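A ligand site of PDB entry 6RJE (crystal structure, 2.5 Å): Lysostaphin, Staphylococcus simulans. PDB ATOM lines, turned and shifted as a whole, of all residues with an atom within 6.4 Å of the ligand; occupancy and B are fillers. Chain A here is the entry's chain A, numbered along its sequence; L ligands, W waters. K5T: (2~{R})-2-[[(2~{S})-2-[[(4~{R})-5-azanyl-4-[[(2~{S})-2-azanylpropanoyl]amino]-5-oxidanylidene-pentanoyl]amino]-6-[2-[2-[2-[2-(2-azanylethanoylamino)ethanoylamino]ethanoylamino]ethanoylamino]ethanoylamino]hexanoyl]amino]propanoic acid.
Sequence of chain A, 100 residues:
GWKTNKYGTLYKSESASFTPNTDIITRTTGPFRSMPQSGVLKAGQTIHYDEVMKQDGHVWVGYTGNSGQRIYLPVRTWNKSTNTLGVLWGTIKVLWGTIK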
ATOM      1  N   THR A   4     -20.505 -25.309  29.571  1.00  0.00           N
ATOM      2  CA  THR A   4     -19.558 -24.817  28.538  1.00  0.00           C
ATOM      3  C   THR A   4     -19.409 -25.893  27.466  1.00  0.00           C
ATOM      4  O   THR A   4     -19.148 -27.055  27.832  1.00  0.00           O
ATOM      5  CB  THR A   4     -18.224 -24.395  29.170  1.00  0.00           C
ATOM      6  OG1 THR A   4     -18.498 -23.447  30.208  1.00  0.00           O
ATOM      7  CG2 THR A   4     -17.258 -23.787  28.178  1.00  0.00           C
ATOM      8  N   ASN A   5     -19.578 -25.524  26.189  1.00  0.00           N
ATOM      9  CA  ASN A   5     -19.508 -26.445  25.024  1.00  0.00           C
ATOM     10  C   ASN A   5     -18.085 -26.420  24.456  1.00  0.00           C
ATOM     11  O   ASN A   5     -17.262 -25.611  24.935  1.00  0.00           O
ATOM     12  CB  ASN A   5     -20.584 -26.114  23.985  1.00  0.00           C
ATOM     13  CG  ASN A   5     -20.332 -24.832  23.216  1.00  0.00           C
ATOM     14  OD1 ASN A   5     -19.369 -24.114  23.482  1.00  0.00           O
ATOM     15  ND2 ASN A   5     -21.193 -24.530  22.261  1.00  0.00           N
ATOM     16  N   LYS A   6     -17.827 -27.275  23.457  1.00  0.00           N
ATOM     17  CA  LYS A   6     -16.534 -27.410  22.732  1.00  0.00           C
ATOM     18  C   LYS A   6     -15.914 -26.035  22.442  1.00  0.00           C
ATOM     19  O   LYS A   6     -14.677 -25.926  22.494  1.00  0.00           O
ATOM     20  CB  LYS A   6     -16.732 -28.122  21.381  1.00  0.00           C
ATOM     21  CG  LYS A   6     -17.219 -29.567  21.458  1.00  0.00           C
ATOM     22  CD  LYS A   6     -17.187 -30.274  20.119  1.00  0.00           C
ATOM     23  CE  LYS A   6     -17.988 -31.564  20.101  1.00  0.00           C
ATOM     24  NZ  LYS A   6     -17.526 -32.515  21.145  1.00  0.00           N
ATOM     25  N   TYR A   7     -16.755 -25.039  22.126  1.00  0.00           N
ATOM     26  CA  TYR A   7     -16.362 -23.754  21.491  1.00  0.00           C
ATOM     27  C   TYR A   7     -16.266 -22.614  22.525  1.00  0.00           C
ATOM     28  O   TYR A   7     -16.071 -21.466  22.098  1.00  0.00           O
ATOM     29  CB  TYR A   7     -17.366 -23.405  20.390  1.00  0.00           C
ATOM     30  CG  TYR A   7     -17.610 -24.520  19.407  1.00  0.00           C
ATOM     31  CD1 TYR A   7     -16.582 -24.990  18.601  1.00  0.00           C
ATOM     32  CD2 TYR A   7     -18.855 -25.124  19.294  1.00  0.00           C
ATOM     33  CE1 TYR A   7     -16.794 -26.023  17.701  1.00  0.00           C
ATOM     34  CE2 TYR A   7     -19.077 -26.163  18.401  1.00  0.00           C
ATOM     35  CZ  TYR A   7     -18.037 -26.606  17.597  1.00  0.00           C
ATOM     36  OH  TYR A   7     -18.246 -27.618  16.705  1.00  0.00           O
ATOM     37  N   GLY A   8     -16.394 -22.933  23.818  1.00  0.00           N
ATOM     38  CA  GLY A   8     -16.276 -21.944  24.910  1.00  0.00           C
ATOM     39  C   GLY A   8     -17.500 -21.065  25.033  1.00  0.00           C
ATOM     40  O   GLY A   8     -17.395 -19.970  25.611  1.00  0.00           O
ATOM     41  N   THR A   9     -18.642 -21.516  24.492  1.00  0.00           N
ATOM     42  CA  THR A   9     -19.967 -20.866  24.660  1.00  0.00           C
ATOM     43  C   THR A   9     -20.574 -21.349  25.980  1.00  0.00           C
ATOM     44  O   THR A   9     -20.722 -22.572  26.151  1.00  0.00           O
ATOM     45  CB  THR A   9     -20.891 -21.171  23.471  1.00  0.00           C
ATOM     46  OG1 THR A   9     -20.280 -20.630  22.296  1.00  0.00           O
ATOM     47  CG2 THR A   9     -22.291 -20.613  23.624  1.00  0.00           C
ATOM     48  N   LEU A  10     -20.877 -20.414  26.878  1.00  0.00           N
ATOM     49  CA  LEU A  10     -21.681 -20.673  28.102  1.00  0.00           C
ATOM     50  C   LEU A  10     -23.138 -20.800  27.672  1.00  0.00           C
ATOM     51  O   LEU A  10     -23.586 -19.944  26.884  1.00  0.00           O
ATOM     52  CB  LEU A  10     -21.470 -19.528  29.094  1.00  0.00           C
ATOM     53  CG  LEU A  10     -20.073 -19.441  29.709  1.00  0.00           C
ATOM     54  CD1 LEU A  10     -19.809 -18.072  30.301  1.00  0.00           C
ATOM     55  CD2 LEU A  10     -19.896 -20.521  30.769  1.00  0.00           C
ATOM     56  N   TYR A  11     -23.833 -21.862  28.112  1.00  0.00           N
ATOM     57  CA  TYR A  11     -25.214 -22.190  27.657  1.00  0.00           C
ATOM     58  C   TYR A  11     -25.977 -22.970  28.737  1.00  0.00           C
ATOM     59  O   TYR A  11     -25.348 -23.562  29.644  1.00  0.00           O
ATOM     60  CB  TYR A  11     -25.175 -22.976  26.351  1.00  0.00           C
ATOM     61  CG  TYR A  11     -24.878 -24.450  26.498  1.00  0.00           C
ATOM     62  CD1 TYR A  11     -23.587 -24.916  26.614  1.00  0.00           C
ATOM     63  CD2 TYR A  11     -25.906 -25.379  26.528  1.00  0.00           C
ATOM     64  CE1 TYR A  11     -23.313 -26.268  26.746  1.00  0.00           C
ATOM     65  CE2 TYR A  11     -25.654 -26.728  26.659  1.00  0.00           C
ATOM     66  CZ  TYR A  11     -24.356 -27.179  26.772  1.00  0.00           C
ATOM     67  OH  TYR A  11     -24.098 -28.512  26.900  1.00  0.00           O
ATOM     68  N   LYS A  12     -27.305 -22.973  28.613  1.00  0.00           N
ATOM     69  CA  LYS A  12     -28.234 -23.728  29.491  1.00  0.00           C
ATOM     70  C   LYS A  12     -29.629 -23.708  28.867  1.00  0.00           C
ATOM     71  O   LYS A  12     -29.855 -22.926  27.905  1.00  0.00           O
ATOM     72  CB  LYS A  12     -28.238 -23.127  30.896  1.00  0.00           C
ATOM     73  CG  LYS A  12     -28.728 -21.682  30.980  1.00  0.00           C
ATOM     74  CD  LYS A  12     -28.671 -21.099  32.372  1.00  0.00           C
ATOM     75  CE  LYS A  12     -29.480 -19.832  32.504  1.00  0.00           C
ATOM     76  NZ  LYS A  12     -29.217 -19.154  33.803  1.00  0.00           N
ATOM     77  N   THR A  29     -26.290 -21.641  12.729  1.00  0.00           N
ATOM     78  CA  THR A  29     -25.081 -22.420  13.063  1.00  0.00           C
ATOM     79  C   THR A  29     -24.714 -22.254  14.545  1.00  0.00           C
ATOM     80  O   THR A  29     -24.609 -23.285  15.236  1.00  0.00           O
ATOM     81  CB  THR A  29     -23.930 -22.034  12.123  1.00  0.00           C
ATOM     82  OG1 THR A  29     -24.492 -21.933  10.814  1.00  0.00           O
ATOM     83  CG2 THR A  29     -22.786 -23.033  12.138  1.00  0.00           C
ATOM     84  N   GLY A  30     -24.511 -21.025  15.026  1.00  0.00           N
ATOM     85  CA  GLY A  30     -24.124 -20.763  16.431  1.00  0.00           C
ATOM     86  C   GLY A  30     -24.175 -19.282  16.801  1.00  0.00           C
ATOM     87  O   GLY A  30     -24.404 -18.428  15.945  1.00  0.00           O
ATOM     88  N   PRO A  31     -23.975 -18.958  18.095  1.00  0.00           N
ATOM     89  CA  PRO A  31     -24.034 -17.574  18.586  1.00  0.00           C
ATOM     90  C   PRO A  31     -22.722 -16.797  18.354  1.00  0.00           C
ATOM     91  O   PRO A  31     -22.009 -16.538  19.307  1.00  0.00           O
ATOM     92  CB  PRO A  31     -24.347 -17.779  20.075  1.00  0.00           C
ATOM     93  CG  PRO A  31     -23.632 -19.054  20.423  1.00  0.00           C
ATOM     94  CD  PRO A  31     -23.746 -19.917  19.190  1.00  0.00           C
ATOM     95  N   PHE A  32     -22.448 -16.457  17.094  1.00  0.00           N
ATOM     96  CA  PHE A  32     -21.321 -15.594  16.663  1.00  0.00           C
ATOM     97  C   PHE A  32     -21.785 -14.722  15.498  1.00  0.00           C
ATOM     98  O   PHE A  32     -22.487 -15.246  14.618  1.00  0.00           O
ATOM     99  CB  PHE A  32     -20.108 -16.429  16.242  1.00  0.00           C
ATOM    100  CG  PHE A  32     -19.563 -17.370  17.286  1.00  0.00           C
ATOM    101  CD1 PHE A  32     -20.140 -18.616  17.494  1.00  0.00           C
ATOM    102  CD2 PHE A  32     -18.440 -17.038  18.025  1.00  0.00           C
ATOM    103  CE1 PHE A  32     -19.628 -19.488  18.445  1.00  0.00           C
ATOM    104  CE2 PHE A  32     -17.928 -17.910  18.975  1.00  0.00           C
ATOM    105  CZ  PHE A  32     -18.520 -19.137  19.179  1.00  0.00           C
ATOM    106  N   MET A  35     -21.030 -15.789  11.985  1.00  0.00           N
ATOM    107  CA  MET A  35     -21.881 -16.858  11.414  1.00  0.00           C
ATOM    108  C   MET A  35     -22.752 -16.272  10.307  1.00  0.00           C
ATOM    109  O   MET A  35     -23.025 -15.080  10.292  1.00  0.00           O
ATOM    110  CB  MET A  35     -22.781 -17.492  12.478  1.00  0.00           C
ATOM    111  CG  MET A  35     -22.029 -18.389  13.440  1.00  0.00           C
ATOM    112  SD  MET A  35     -21.068 -19.674  12.606  1.00  0.00           S
ATOM    113  CE  MET A  35     -20.330 -20.499  14.012  1.00  0.00           C
ATOM    114  N   GLU A  51     -33.418 -22.052  24.727  1.00  0.00           N
ATOM    115  CA  GLU A  51     -31.973 -22.048  25.049  1.00  0.00           C
ATOM    116  C   GLU A  51     -31.488 -20.609  25.275  1.00  0.00           C
ATOM    117  O   GLU A  51     -32.078 -19.695  24.663  1.00  0.00           O
ATOM    118  CB  GLU A  51     -31.194 -22.729  23.922  1.00  0.00           C
ATOM    119  CG  GLU A  51     -29.784 -23.152  24.307  1.00  0.00           C
ATOM    120  CD  GLU A  51     -29.049 -23.942  23.238  1.00  0.00           C
ATOM    121  OE1 GLU A  51     -29.206 -23.632  22.035  1.00  0.00           O
ATOM    122  OE2 GLU A  51     -28.324 -24.880  23.612  1.00  0.00           O
ATOM    123  N   VAL A  52     -30.489 -20.423  26.147  1.00  0.00           N
ATOM    124  CA  VAL A  52     -29.792 -19.117  26.369  1.00  0.00           C
ATOM    125  C   VAL A  52     -28.281 -19.359  26.394  1.00  0.00           C
ATOM    126  O   VAL A  52     -27.848 -20.317  27.050  1.00  0.00           O
ATOM    127  CB  VAL A  52     -30.281 -18.421  27.661  1.00  0.00           C
ATOM    128  CG1 VAL A  52     -29.528 -17.126  27.938  1.00  0.00           C
ATOM    129  CG2 VAL A  52     -31.780 -18.169  27.620  1.00  0.00           C
ATOM    130  N   MET A  53     -27.533 -18.495  25.699  1.00  0.00           N
ATOM    131  CA  MET A  53     -26.054 -18.619  25.510  1.00  0.00           C
ATOM    132  C   MET A  53     -25.366 -17.274  25.769  1.00  0.00           C
ATOM    133  O   MET A  53     -25.935 -16.221  25.405  1.00  0.00           O
ATOM    134  CB  MET A  53     -25.750 -19.055  24.072  1.00  0.00           C
ATOM    135  CG  MET A  53     -26.159 -20.484  23.780  1.00  0.00           C
ATOM    136  SD  MET A  53     -26.730 -20.673  22.095  1.00  0.00           S
ATOM    137  CE  MET A  53     -28.408 -20.069  22.232  1.00  0.00           C
ATOM    138  N   TYR A  72     -30.065 -18.278  16.064  1.00  0.00           N
ATOM    139  CA  TYR A  72     -29.354 -17.663  17.214  1.00  0.00           C
ATOM    140  C   TYR A  72     -29.594 -16.142  17.179  1.00  0.00           C
ATOM    141  O   TYR A  72     -29.170 -15.462  16.222  1.00  0.00           O
ATOM    142  CB  TYR A  72     -27.887 -18.093  17.209  1.00  0.00           C
ATOM    143  CG  TYR A  72     -27.726 -19.586  17.324  1.00  0.00           C
ATOM    144  CD1 TYR A  72     -27.775 -20.400  16.205  1.00  0.00           C
ATOM    145  CD2 TYR A  72     -27.600 -20.204  18.556  1.00  0.00           C
ATOM    146  CE1 TYR A  72     -27.666 -21.778  16.300  1.00  0.00           C
ATOM    147  CE2 TYR A  72     -27.496 -21.582  18.672  1.00  0.00           C
ATOM    148  CZ  TYR A  72     -27.527 -22.373  17.543  1.00  0.00           C
ATOM    149  OH  TYR A  72     -27.419 -23.723  17.650  1.00  0.00           O
HETATM  150  C10 K5T L   1     -23.390 -24.612  18.570  1.00  0.00           C
HETATM  151  N12 K5T L   1     -25.051 -24.509  20.317  1.00  0.00           N
HETATM  152  C13 K5T L   1     -24.585 -23.635  21.348  1.00  0.00           C
HETATM  153  C17 K5T L   1     -25.987 -27.590  23.144  1.00  0.00           C
HETATM  154  C24 K5T L   1     -14.210 -28.362  11.221  1.00  0.00           C
HETATM  155  C28 K5T L   1     -13.468 -28.463  12.535  1.00  0.00           C
HETATM  156  C01 K5T L   1     -15.521 -21.916  13.882  1.00  0.00           C
HETATM  157  N02 K5T L   1     -16.536 -21.744  14.845  1.00  0.00           N
HETATM  158  C03 K5T L   1     -17.551 -22.731  15.036  1.00  0.00           C
HETATM  159  C04 K5T L   1     -18.637 -22.527  16.083  1.00  0.00           C
HETATM  160  N05 K5T L   1     -19.545 -23.609  16.069  1.00  0.00           N
HETATM  161  C06 K5T L   1     -20.710 -23.607  16.880  1.00  0.00           C
HETATM  162  O07 K5T L   1     -20.937 -22.655  17.606  1.00  0.00           O
HETATM  163  C08 K5T L   1     -21.645 -24.792  16.840  1.00  0.00           C
HETATM  164  N09 K5T L   1     -22.964 -24.434  17.233  1.00  0.00           N
HETATM  165  C11 K5T L   1     -24.807 -24.211  18.960  1.00  0.00           C
HETATM  166  C14 K5T L   1     -24.829 -23.940  22.811  1.00  0.00           C
HETATM  167  N15 K5T L   1     -25.628 -25.106  22.946  1.00  0.00           N
HETATM  168  C16 K5T L   1     -25.054 -26.401  22.999  1.00  0.00           C
HETATM  169  N18 K5T L   1     -25.320 -28.809  23.447  1.00  0.00           N
HETATM  170  O19 K5T L   1     -23.843 -26.545  22.940  1.00  0.00           O
HETATM  171  O20 K5T L   1     -23.980 -22.628  21.050  1.00  0.00           O
HETATM  172  O21 K5T L   1     -22.642 -25.080  19.399  1.00  0.00           O
HETATM  173  O22 K5T L   1     -17.552 -23.746  14.360  1.00  0.00           O
HETATM  174  C23 K5T L   1     -14.150 -21.941  14.523  1.00  0.00           C
HETATM  175  O25 K5T L   1     -14.676 -29.954  13.989  1.00  0.00           O
HETATM  176  O26 K5T L   1     -12.864 -30.732  13.058  1.00  0.00           O
HETATM  177  C27 K5T L   1     -13.682 -29.780  13.227  1.00  0.00           C
HETATM  178  N29 K5T L   1     -13.819 -27.370  13.388  1.00  0.00           N
HETATM  179  O30 K5T L   1     -11.763 -27.251  14.405  1.00  0.00           O
HETATM  180  C31 K5T L   1     -12.889 -26.820  14.311  1.00  0.00           C
HETATM  181  O32 K5T L   1     -13.597 -27.072  17.589  1.00  0.00           O
HETATM  182  N33 K5T L   1      -8.982 -27.556  20.792  1.00  0.00           N
HETATM  183  O34 K5T L   1     -10.907 -28.785  20.839  1.00  0.00           O
HETATM  184  C35 K5T L   1     -10.391 -27.685  20.911  1.00  0.00           C
HETATM  185  O36 K5T L   1      -9.967 -25.948  23.544  1.00  0.00           O
HETATM  186  C37 K5T L   1     -12.309 -27.886  25.181  1.00  0.00           C
HETATM  187  N38 K5T L   1     -12.809 -25.501  25.133  1.00  0.00           N
HETATM  188  C39 K5T L   1     -11.786 -26.481  24.949  1.00  0.00           C
HETATM  189  C40 K5T L   1     -11.118 -26.316  23.596  1.00  0.00           C
HETATM  190  N41 K5T L   1     -11.858 -26.597  22.412  1.00  0.00           N
HETATM  191  C42 K5T L   1     -11.250 -26.460  21.129  1.00  0.00           C
HETATM  192  C43 K5T L   1     -12.297 -26.290  20.034  1.00  0.00           C
HETATM  193  C44 K5T L   1     -11.687 -26.129  18.663  1.00  0.00           C
HETATM  194  C45 K5T L   1     -12.657 -26.305  17.504  1.00  0.00           C
HETATM  195  N46 K5T L   1     -12.441 -25.548  16.320  1.00  0.00           N
HETATM  196  C47 K5T L   1     -13.309 -25.663  15.196  1.00  0.00           C
HETATM  197  C48 K5T L   1     -13.351 -24.348  14.458  1.00  0.00           C
HETATM  198  C49 K5T L   1     -13.882 -23.217  15.299  1.00  0.00           C
HETATM  199  O   HOH W   1     -26.371 -27.426  19.236  1.00  0.00           O
HETATM  200  O   HOH W   2     -10.752 -31.121  11.644  1.00  0.00           O
HETATM  201  O   HOH W   3     -21.460 -22.364  20.414  1.00  0.00           O
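The side-chain amide oxygen (OD1) of Asn 5 sits close to the backbone NH (N) of Tyr 7, at 3.1 Å.
OD1 of Asn 5 lies within hydrogen-bond range of N of Thr 9 (2.9 Å).
The backbone NH (N) of Gly 8 lies within hydrogen-bond range of the side-chain amide oxygen (OD1) of Asn 5 (3.2 Å).
O20 of the ligand lies close to SD of Met 53.
Residues that only touch the ligand: Tyr 7 (3.3 Å), Thr 9 (3.7 Å), Tyr 11 (3.6 Å), Gly 30 (3.9 Å), Pro 31 (3.3 Å), Phe 32 (3.5 Å), Met 35 (3.4 Å) and Tyr 72 (3.0 Å).
Hydrophobic or aromatic side chains within 4 Å of the ligand: Tyr 7, Tyr 11, Pro 31, Phe 32, Met 35, Met 53 and Tyr 72.
Of the 18 residues printed, 13 come within 4 Å of the ligand.
Water W3 lies within hydrogen-bond range of O20 of the ligand (2.6 Å), OG1 of Thr 9 (2.8 Å) and ND2 of Asn 5 (2.9 Å).
OE2 of Glu 51 is in hydrogen-bond range of N15 of the ligand (2.8 Å).
O of Thr 29 is in hydrogen-bond range of N09 of the ligand (2.8 Å).
A nitrogen (N41) of the ligand is in hydrogen-bond range of the backbone carbonyl oxygen (O) of Lys 6 (2.9 Å).
ND2 of Asn 5 sits at hydrogen-bond distance from O21 of the ligand.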
